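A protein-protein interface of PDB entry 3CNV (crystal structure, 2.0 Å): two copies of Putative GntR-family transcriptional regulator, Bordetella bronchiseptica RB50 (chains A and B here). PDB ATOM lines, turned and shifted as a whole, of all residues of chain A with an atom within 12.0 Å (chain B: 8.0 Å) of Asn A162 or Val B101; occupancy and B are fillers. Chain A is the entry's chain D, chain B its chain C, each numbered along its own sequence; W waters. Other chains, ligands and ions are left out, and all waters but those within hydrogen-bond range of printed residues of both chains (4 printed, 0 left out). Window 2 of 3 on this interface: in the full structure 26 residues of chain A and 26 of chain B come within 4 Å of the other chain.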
ATOM      1  N   ARG A   7      39.571  37.391 -15.673  1.00  0.00           N
ATOM      2  CA  ARG A   7      38.098  37.219 -15.697  1.00  0.00           C
ATOM      3  C   ARG A   7      37.391  38.511 -16.045  1.00  0.00           C
ATOM      4  O   ARG A   7      36.174  38.573 -16.008  1.00  0.00           O
ATOM      5  CB  ARG A   7      37.547  36.715 -14.386  1.00  0.00           C
ATOM      6  CG  ARG A   7      37.963  35.296 -14.068  1.00  0.00           C
ATOM      7  CD  ARG A   7      37.438  34.290 -15.059  1.00  0.00           C
ATOM      8  NE  ARG A   7      37.844  32.979 -14.600  1.00  0.00           N
ATOM      9  CZ  ARG A   7      37.206  32.365 -13.608  1.00  0.00           C
ATOM     10  NH1 ARG A   7      36.195  33.000 -12.977  1.00  0.00           N
ATOM     11  NH2 ARG A   7      37.557  31.146 -13.221  1.00  0.00           N
ATOM     12  N   ARG A 158      33.979  38.095 -14.223  1.00  0.00           N
ATOM     13  CA  ARG A 158      32.967  37.054 -14.564  1.00  0.00           C
ATOM     14  C   ARG A 158      33.319  35.753 -13.880  1.00  0.00           C
ATOM     15  O   ARG A 158      34.496  35.369 -13.783  1.00  0.00           O
ATOM     16  CB  ARG A 158      32.819  36.871 -16.071  1.00  0.00           C
ATOM     17  CG  ARG A 158      33.986  36.166 -16.692  1.00  0.00           C
ATOM     18  CD  ARG A 158      33.676  35.699 -18.121  1.00  0.00           C
ATOM     19  NE  ARG A 158      34.918  35.448 -18.860  1.00  0.00           N
ATOM     20  CZ  ARG A 158      35.808  34.464 -18.618  1.00  0.00           C
ATOM     21  NH1 ARG A 158      35.665  33.578 -17.606  1.00  0.00           N
ATOM     22  NH2 ARG A 158      36.870  34.400 -19.404  1.00  0.00           N
ATOM     23  N   ASN A 159      32.323  35.137 -13.286  1.00  0.00           N
ATOM     24  CA  ASN A 159      32.521  33.875 -12.629  1.00  0.00           C
ATOM     25  C   ASN A 159      31.314  32.965 -12.762  1.00  0.00           C
ATOM     26  O   ASN A 159      30.215  33.327 -12.403  1.00  0.00           O
ATOM     27  CB  ASN A 159      32.825  34.081 -11.122  1.00  0.00           C
ATOM     28  CG  ASN A 159      33.429  32.823 -10.443  1.00  0.00           C
ATOM     29  OD1 ASN A 159      34.205  32.086 -11.054  1.00  0.00           O
ATOM     30  ND2 ASN A 159      33.148  32.642  -9.160  1.00  0.00           N
ATOM     31  N   SER A 160      31.564  31.736 -13.170  1.00  0.00           N
ATOM     32  CA  SER A 160      30.565  30.700 -13.167  1.00  0.00           C
ATOM     33  C   SER A 160      30.832  29.708 -12.069  1.00  0.00           C
ATOM     34  O   SER A 160      31.968  29.286 -11.885  1.00  0.00           O
ATOM     35  CB  SER A 160      30.508  29.950 -14.492  1.00  0.00           C
ATOM     36  OG  SER A 160      30.066  30.850 -15.477  1.00  0.00           O
ATOM     37  N   LEU A 161      29.773  29.397 -11.353  1.00  0.00           N
ATOM     38  CA  LEU A 161      29.791  28.494 -10.214  1.00  0.00           C
ATOM     39  C   LEU A 161      28.979  27.251 -10.495  1.00  0.00           C
ATOM     40  O   LEU A 161      27.864  27.376 -11.020  1.00  0.00           O
ATOM     41  CB  LEU A 161      29.193  29.174  -8.961  1.00  0.00           C
ATOM     42  CG  LEU A 161      29.415  30.651  -8.593  1.00  0.00           C
ATOM     43  CD1 LEU A 161      29.431  30.904  -7.004  1.00  0.00           C
ATOM     44  CD2 LEU A 161      30.500  31.345  -9.293  1.00  0.00           C
ATOM     45  N   ASN A 162      29.535  26.086 -10.177  1.00  0.00           N
ATOM     46  CA  ASN A 162      28.807  24.844 -10.197  1.00  0.00           C
ATOM     47  C   ASN A 162      28.033  24.534  -8.885  1.00  0.00           C
ATOM     48  O   ASN A 162      27.350  23.477  -8.765  1.00  0.00           O
ATOM     49  CB  ASN A 162      29.761  23.710 -10.358  1.00  0.00           C
ATOM     50  CG  ASN A 162      30.434  23.712 -11.685  1.00  0.00           C
ATOM     51  OD1 ASN A 162      29.811  23.353 -12.636  1.00  0.00           O
ATOM     52  ND2 ASN A 162      31.704  24.136 -11.750  1.00  0.00           N
ATOM     53  OXT ASN A 162      28.188  25.233  -7.901  1.00  0.00           O
ATOM     54  N   ARG B   4      25.043  26.892  -0.798  1.00  0.00           N
ATOM     55  CA  ARG B   4      24.967  26.505  -2.166  1.00  0.00           C
ATOM     56  C   ARG B   4      26.000  27.296  -2.961  1.00  0.00           C
ATOM     57  O   ARG B   4      26.845  26.701  -3.744  1.00  0.00           O
ATOM     58  CB  ARG B   4      23.532  26.704  -2.722  1.00  0.00           C
ATOM     59  CG  ARG B   4      23.407  26.400  -4.190  1.00  0.00           C
ATOM     60  CD  ARG B   4      23.540  24.972  -4.383  1.00  0.00           C
ATOM     61  NE  ARG B   4      23.621  24.528  -5.786  1.00  0.00           N
ATOM     62  CZ  ARG B   4      24.745  24.464  -6.482  1.00  0.00           C
ATOM     63  NH1 ARG B   4      25.923  24.765  -5.949  1.00  0.00           N
ATOM     64  NH2 ARG B   4      24.702  24.056  -7.723  1.00  0.00           N
ATOM     65  N   PHE B   5      25.949  28.609  -2.834  1.00  0.00           N
ATOM     66  CA  PHE B   5      26.810  29.441  -3.703  1.00  0.00           C
ATOM     67  C   PHE B   5      27.662  30.439  -3.009  1.00  0.00           C
ATOM     68  O   PHE B   5      28.599  30.978  -3.587  1.00  0.00           O
ATOM     69  CB  PHE B   5      26.012  30.209  -4.734  1.00  0.00           C
ATOM     70  CG  PHE B   5      25.387  29.356  -5.784  1.00  0.00           C
ATOM     71  CD1 PHE B   5      26.154  28.505  -6.545  1.00  0.00           C
ATOM     72  CD2 PHE B   5      24.036  29.481  -6.080  1.00  0.00           C
ATOM     73  CE1 PHE B   5      25.609  27.775  -7.515  1.00  0.00           C
ATOM     74  CE2 PHE B   5      23.469  28.718  -7.146  1.00  0.00           C
ATOM     75  CZ  PHE B   5      24.242  27.849  -7.810  1.00  0.00           C
ATOM     76  N   ARG B   7      30.342  32.457  -1.217  1.00  0.00           N
ATOM     77  CA  ARG B   7      31.797  32.261  -1.252  1.00  0.00           C
ATOM     78  C   ARG B   7      32.505  33.107  -0.189  1.00  0.00           C
ATOM     79  O   ARG B   7      33.712  33.198  -0.114  1.00  0.00           O
ATOM     80  CB  ARG B   7      32.354  32.624  -2.652  1.00  0.00           C
ATOM     81  CG  ARG B   7      31.978  31.704  -3.729  1.00  0.00           C
ATOM     82  CD  ARG B   7      32.408  30.268  -3.395  1.00  0.00           C
ATOM     83  NE  ARG B   7      32.077  29.545  -4.554  1.00  0.00           N
ATOM     84  CZ  ARG B   7      32.675  29.727  -5.740  1.00  0.00           C
ATOM     85  NH1 ARG B   7      33.654  30.647  -5.884  1.00  0.00           N
ATOM     86  NH2 ARG B   7      32.246  29.035  -6.786  1.00  0.00           N
ATOM     87  N   GLU B  93      14.540  24.480  -2.597  1.00  0.00           N
ATOM     88  CA  GLU B  93      14.626  23.040  -2.911  1.00  0.00           C
ATOM     89  C   GLU B  93      13.488  22.271  -2.281  1.00  0.00           C
ATOM     90  O   GLU B  93      12.702  21.594  -2.964  1.00  0.00           O
ATOM     91  CB  GLU B  93      15.965  22.395  -2.434  1.00  0.00           C
ATOM     92  CG  GLU B  93      17.066  22.458  -3.425  1.00  0.00           C
ATOM     93  CD  GLU B  93      18.463  21.907  -2.956  1.00  0.00           C
ATOM     94  OE1 GLU B  93      18.579  21.373  -1.814  1.00  0.00           O
ATOM     95  OE2 GLU B  93      19.444  22.053  -3.774  1.00  0.00           O
ATOM     96  N   VAL B  98      12.904  23.530  -6.412  1.00  0.00           N
ATOM     97  CA  VAL B  98      13.860  24.220  -7.303  1.00  0.00           C
ATOM     98  C   VAL B  98      15.306  24.066  -6.831  1.00  0.00           C
ATOM     99  O   VAL B  98      15.668  24.584  -5.809  1.00  0.00           O
ATOM    100  CB  VAL B  98      13.433  25.692  -7.414  1.00  0.00           C
ATOM    101  CG1 VAL B  98      14.471  26.512  -8.192  1.00  0.00           C
ATOM    102  CG2 VAL B  98      12.024  25.747  -8.032  1.00  0.00           C
ATOM    103  N   SER B  99      16.108  23.265  -7.562  1.00  0.00           N
ATOM    104  CA  SER B  99      17.516  23.011  -7.231  1.00  0.00           C
ATOM    105  C   SER B  99      18.383  23.621  -8.288  1.00  0.00           C
ATOM    106  O   SER B  99      18.210  23.369  -9.463  1.00  0.00           O
ATOM    107  CB  SER B  99      17.923  21.529  -7.228  1.00  0.00           C
ATOM    108  OG  SER B  99      17.134  20.760  -6.370  1.00  0.00           O
ATOM    109  N   MET B 100      19.294  24.452  -7.835  1.00  0.00           N
ATOM    110  CA  MET B 100      20.222  25.151  -8.742  1.00  0.00           C
ATOM    111  C   MET B 100      21.451  24.280  -9.079  1.00  0.00           C
ATOM    112  O   MET B 100      22.180  23.736  -8.195  1.00  0.00           O
ATOM    113  CB  MET B 100      20.659  26.459  -8.130  1.00  0.00           C
ATOM    114  CG  MET B 100      19.579  27.308  -7.517  1.00  0.00           C
ATOM    115  SD  MET B 100      18.207  27.773  -8.839  1.00  0.00           S
ATOM    116  CE  MET B 100      17.086  28.899  -7.601  1.00  0.00           C
ATOM    117  N   VAL B 101      21.715  24.168 -10.370  1.00  0.00           N
ATOM    118  CA  VAL B 101      22.846  23.429 -10.867  1.00  0.00           C
ATOM    119  C   VAL B 101      24.029  24.312 -11.224  1.00  0.00           C
ATOM    120  O   VAL B 101      25.178  23.871 -11.186  1.00  0.00           O
ATOM    121  CB  VAL B 101      22.416  22.557 -12.117  1.00  0.00           C
ATOM    122  CG1 VAL B 101      21.228  21.727 -11.748  1.00  0.00           C
ATOM    123  CG2 VAL B 101      22.067  23.431 -13.269  1.00  0.00           C
ATOM    124  N   ARG B 102      23.755  25.574 -11.528  1.00  0.00           N
ATOM    125  CA  ARG B 102      24.777  26.532 -11.915  1.00  0.00           C
ATOM    126  C   ARG B 102      24.383  27.914 -11.516  1.00  0.00           C
ATOM    127  O   ARG B 102      23.202  28.259 -11.516  1.00  0.00           O
ATOM    128  CB  ARG B 102      24.935  26.572 -13.501  1.00  0.00           C
ATOM    129  CG  ARG B 102      26.195  27.330 -13.960  1.00  0.00           C
ATOM    130  CD  ARG B 102      26.311  27.392 -15.517  1.00  0.00           C
ATOM    131  NE  ARG B 102      25.689  28.551 -16.172  1.00  0.00           N
ATOM    132  CZ  ARG B 102      24.624  28.433 -16.948  1.00  0.00           C
ATOM    133  NH1 ARG B 102      24.096  27.240 -17.132  1.00  0.00           N
ATOM    134  NH2 ARG B 102      24.098  29.470 -17.573  1.00  0.00           N
ATOM    135  N   ALA B 103      25.383  28.748 -11.365  1.00  0.00           N
ATOM    136  CA  ALA B 103      25.191  30.211 -11.204  1.00  0.00           C
ATOM    137  C   ALA B 103      26.198  30.996 -12.038  1.00  0.00           C
ATOM    138  O   ALA B 103      27.375  30.637 -12.115  1.00  0.00           O
ATOM    139  CB  ALA B 103      25.258  30.674  -9.774  1.00  0.00           C
ATOM    140  N   ASP B 104      25.746  32.043 -12.718  1.00  0.00           N
ATOM    141  CA  ASP B 104      26.663  32.882 -13.497  1.00  0.00           C
ATOM    142  C   ASP B 104      26.677  34.227 -12.724  1.00  0.00           C
ATOM    143  O   ASP B 104      25.633  34.763 -12.386  1.00  0.00           O
ATOM    144  CB  ASP B 104      26.197  33.115 -14.908  1.00  0.00           C
ATOM    145  CG  ASP B 104      26.234  31.856 -15.795  1.00  0.00           C
ATOM    146  OD1 ASP B 104      27.029  30.883 -15.511  1.00  0.00           O
ATOM    147  OD2 ASP B 104      25.463  31.865 -16.820  1.00  0.00           O
ATOM    148  N   SER B 135      20.948  32.352 -11.281  1.00  0.00           N
ATOM    149  CA  SER B 135      21.029  30.933 -10.936  1.00  0.00           C
ATOM    150  C   SER B 135      20.089  30.163 -11.813  1.00  0.00           C
ATOM    151  O   SER B 135      18.967  30.600 -12.166  1.00  0.00           O
ATOM    152  CB  SER B 135      20.604  30.667  -9.470  1.00  0.00           C
ATOM    153  OG  SER B 135      21.358  31.471  -8.670  1.00  0.00           O
ATOM    154  N   TYR B 136      20.562  28.989 -12.176  1.00  0.00           N
ATOM    155  CA  TYR B 136      19.896  28.136 -13.150  1.00  0.00           C
ATOM    156  C   TYR B 136      19.554  26.769 -12.568  1.00  0.00           C
ATOM    157  O   TYR B 136      20.278  26.207 -11.768  1.00  0.00           O
ATOM    158  CB  TYR B 136      20.769  27.959 -14.432  1.00  0.00           C
ATOM    159  CG  TYR B 136      21.045  29.236 -15.187  1.00  0.00           C
ATOM    160  CD1 TYR B 136      20.273  29.594 -16.256  1.00  0.00           C
ATOM    161  CD2 TYR B 136      22.063  30.100 -14.805  1.00  0.00           C
ATOM    162  CE1 TYR B 136      20.480  30.801 -16.920  1.00  0.00           C
ATOM    163  CE2 TYR B 136      22.299  31.300 -15.491  1.00  0.00           C
ATOM    164  CZ  TYR B 136      21.476  31.651 -16.504  1.00  0.00           C
ATOM    165  OH  TYR B 136      21.629  32.840 -17.201  1.00  0.00           O
ATOM    166  N   THR B 137      18.410  26.263 -12.967  1.00  0.00           N
ATOM    167  CA  THR B 137      18.057  24.895 -12.708  1.00  0.00           C
ATOM    168  C   THR B 137      18.432  24.131 -13.970  1.00  0.00           C
ATOM    169  O   THR B 137      18.902  24.697 -14.974  1.00  0.00           O
ATOM    170  CB  THR B 137      16.526  24.694 -12.365  1.00  0.00           C
ATOM    171  OG1 THR B 137      15.676  25.042 -13.488  1.00  0.00           O
ATOM    172  CG2 THR B 137      16.104  25.551 -11.213  1.00  0.00           C
ATOM    173  N   TYR B 138      18.215  22.849 -13.914  1.00  0.00           N
ATOM    174  CA  TYR B 138      18.276  21.973 -15.135  1.00  0.00           C
ATOM    175  C   TYR B 138      17.709  22.526 -16.471  1.00  0.00           C
ATOM    176  O   TYR B 138      16.647  23.114 -16.568  1.00  0.00           O
ATOM    177  CB  TYR B 138      17.739  20.561 -14.745  1.00  0.00           C
ATOM    178  CG  TYR B 138      18.759  19.879 -13.790  1.00  0.00           C
ATOM    179  CD1 TYR B 138      19.979  19.352 -14.283  1.00  0.00           C
ATOM    180  CD2 TYR B 138      18.539  19.787 -12.430  1.00  0.00           C
ATOM    181  CE1 TYR B 138      20.939  18.756 -13.434  1.00  0.00           C
ATOM    182  CE2 TYR B 138      19.505  19.201 -11.554  1.00  0.00           C
ATOM    183  CZ  TYR B 138      20.706  18.687 -12.069  1.00  0.00           C
ATOM    184  OH  TYR B 138      21.684  18.116 -11.251  1.00  0.00           O
ATOM    185  N   GLY B 139      18.479  22.311 -17.511  1.00  0.00           N
ATOM    186  CA  GLY B 139      18.048  22.703 -18.829  1.00  0.00           C
ATOM    187  C   GLY B 139      18.339  24.159 -19.063  1.00  0.00           C
ATOM    188  O   GLY B 139      17.767  24.769 -19.962  1.00  0.00           O
ATOM    189  N   ASP B 140      19.210  24.716 -18.238  1.00  0.00           N
ATOM    190  CA  ASP B 140      19.624  26.149 -18.340  1.00  0.00           C
ATOM    191  C   ASP B 140      18.464  27.131 -18.155  1.00  0.00           C
ATOM    192  O   ASP B 140      18.320  28.170 -18.887  1.00  0.00           O
ATOM    193  CB  ASP B 140      20.318  26.417 -19.692  1.00  0.00           C
ATOM    194  CG  ASP B 140      21.738  25.930 -19.688  1.00  0.00           C
ATOM    195  OD1 ASP B 140      22.425  26.198 -18.676  1.00  0.00           O
ATOM    196  OD2 ASP B 140      22.134  25.257 -20.651  1.00  0.00           O
ATOM    197  N   ARG B 141      17.559  26.725 -17.274  1.00  0.00           N
ATOM    198  CA  ARG B 141      16.381  27.547 -16.967  1.00  0.00           C
ATOM    199  C   ARG B 141      16.709  28.506 -15.846  1.00  0.00           C
ATOM    200  O   ARG B 141      17.035  28.059 -14.768  1.00  0.00           O
ATOM    201  CB  ARG B 141      15.216  26.697 -16.551  1.00  0.00           C
ATOM    202  CG  ARG B 141      14.660  25.944 -17.707  1.00  0.00           C
ATOM    203  CD  ARG B 141      13.573  24.983 -17.274  1.00  0.00           C
ATOM    204  NE  ARG B 141      12.905  24.435 -18.453  1.00  0.00           N
ATOM    205  CZ  ARG B 141      13.392  23.493 -19.264  1.00  0.00           C
ATOM    206  NH1 ARG B 141      14.563  22.914 -19.023  1.00  0.00           N
ATOM    207  NH2 ARG B 141      12.669  23.102 -20.308  1.00  0.00           N
ATOM    208  N   SER B 160      38.306  29.370  -6.521  1.00  0.00           N
ATOM    209  CA  SER B 160      39.321  28.538  -7.158  1.00  0.00           C
ATOM    210  C   SER B 160      39.034  28.475  -8.622  1.00  0.00           C
ATOM    211  O   SER B 160      37.860  28.314  -9.044  1.00  0.00           O
ATOM    212  CB  SER B 160      39.306  27.090  -6.626  1.00  0.00           C
ATOM    213  OG  SER B 160      39.814  27.082  -5.308  1.00  0.00           O
ATOM    214  N   ASN B 162      40.279  26.839 -12.468  1.00  0.00           N
ATOM    215  CA  ASN B 162      40.900  25.778 -13.194  1.00  0.00           C
ATOM    216  C   ASN B 162      41.659  26.399 -14.378  1.00  0.00           C
ATOM    217  O   ASN B 162      41.596  27.599 -14.588  1.00  0.00           O
ATOM    218  CB  ASN B 162      39.869  24.808 -13.702  1.00  0.00           C
ATOM    219  CG  ASN B 162      39.260  23.950 -12.578  1.00  0.00           C
ATOM    220  OD1 ASN B 162      39.834  22.996 -12.188  1.00  0.00           O
ATOM    221  ND2 ASN B 162      38.076  24.282 -12.139  1.00  0.00           N
ATOM    222  OXT ASN B 162      42.397  25.708 -15.112  1.00  0.00           O
HETATM  223  O   HOH W   1      36.300  29.641 -10.841  1.00  0.00           O
HETATM  224  O   HOH W   2      27.412  22.840 -13.198  1.00  0.00           O
HETATM  225  O   HOH W   3      33.724  29.424  -9.463  1.00  0.00           O
HETATM  226  O   HOH W   4      39.705  29.118 -14.896  1.00  0.00           O
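N of Leu A161 is in hydrogen-bond range of O of Ala B103 (2.8 Å).
The side-chain carboxylate (OD1) of Asp B104 is in hydrogen-bond range of the side-chain hydroxyl (OG) of Ser A160, 3.0 Å away.
The backbone carbonyl oxygen (O) of Val B101 sits close to the chain-end carboxylate (O) of Asn A162.
NH2 of Arg B4 lies within salt-bridge range of O of Asn A162 (2.9 Å).
O of Tyr B136 sits at hydrogen-bond distance from N of Val B101 (2.9 Å).
The guanidinium group of Arg A7 sits at hydrogen-bond distance from the side-chain amide oxygen of Asn A159, 2.9 Å away.
The side-chain carboxylate of Asp B104 lies within salt-bridge range of the guanidinium group of Arg B102, at 2.8 Å.
The guanidinium group (NH1) of Arg B102 lies within salt-bridge range of the side-chain carboxylate (OD1) of Asp B140 (2.5 Å).
O of Met B100 sits at hydrogen-bond distance from NH2 of Arg B4.
N of Tyr B136 sits at hydrogen-bond distance from O of Arg B102, 2.8 Å away.
Among the printed residues, pairs that only touch across the chains: Asn A159 with Arg B7, Asn A159 with Ala B103, Asn A159 with Asp B104, Ser A160 with Ala B103, Leu A161 with Phe B5, Leu A161 with Arg B7, Leu A161 with Arg B102 and Asn A162 with Phe B5.
Of chain B, only Arg B4 (2.9 Å), Phe B5 (3.6 Å) and Val B101 (3.3 Å) come within 4 Å of Asn A162.
Val B101 touches one residue of chain A.
No residue of chain A comes within 4 Å of Ser B99.
No residue of chain A comes within 4 Å of Met B100.
Ala B103 touches three residues of chain A.
No residue of chain A comes within 4 Å of Thr B137.
Printed residues of chain A within 4 Å of Arg B7: Asn A159 and Leu A161.
Printed residues of chain B within 4 Å of Ser A160: Ala B103 and Asp B104.
Of the printed residues of chain A, Asp B104 touches Asn A159 and Ser A160.
Arg A158 touches none of the printed residues of chain B.
The nearest residue of chain B that does not touch Asn A162 is Arg B102 (4.7 Å).
Printed residues of chain B that touch a printed residue of chain A: Arg B4, Phe B5, Arg B7, Val B101, Arg B102, Ala B103 and Asp B104.
Of the 6 printed residues of chain A, 4 touch a printed residue of chain B.
Among the printed residues, 12 pairs touch across the chains.
Among the printed residues, no Asp or Glu carboxylate lies within 4 Å of a Lys or Arg side-chain nitrogen of the other chain.
Positions printed for both chains: 7, 160 and 162.
Of the 12 pairs that touch across the chains among the printed residues, none has its exchanged pair printed and touching as well.
Water W4 lies within hydrogen-bond range of O of Asn B162 (2.4 Å) and NH2 of Arg A7 (3.4 Å).
Water W2 bridges OD1 of Asn A162 (2.5 Å) and O of Val B101 (3.2 Å).
Water W1 lies within hydrogen-bond range of the backbone carbonyl oxygen (O) of Ser B160 (2.7 Å), the guanidinium group (NH2) of Arg A7 (3.1 Å) and the side-chain amide oxygen (OD1) of Asn A159 (3.2 Å).
Water W3 lies within hydrogen-bond range of O of Ser A160 (3.0 Å), NH2 of Arg B7 (3.1 Å) and OD1 of Asn A159 (3.1 Å).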
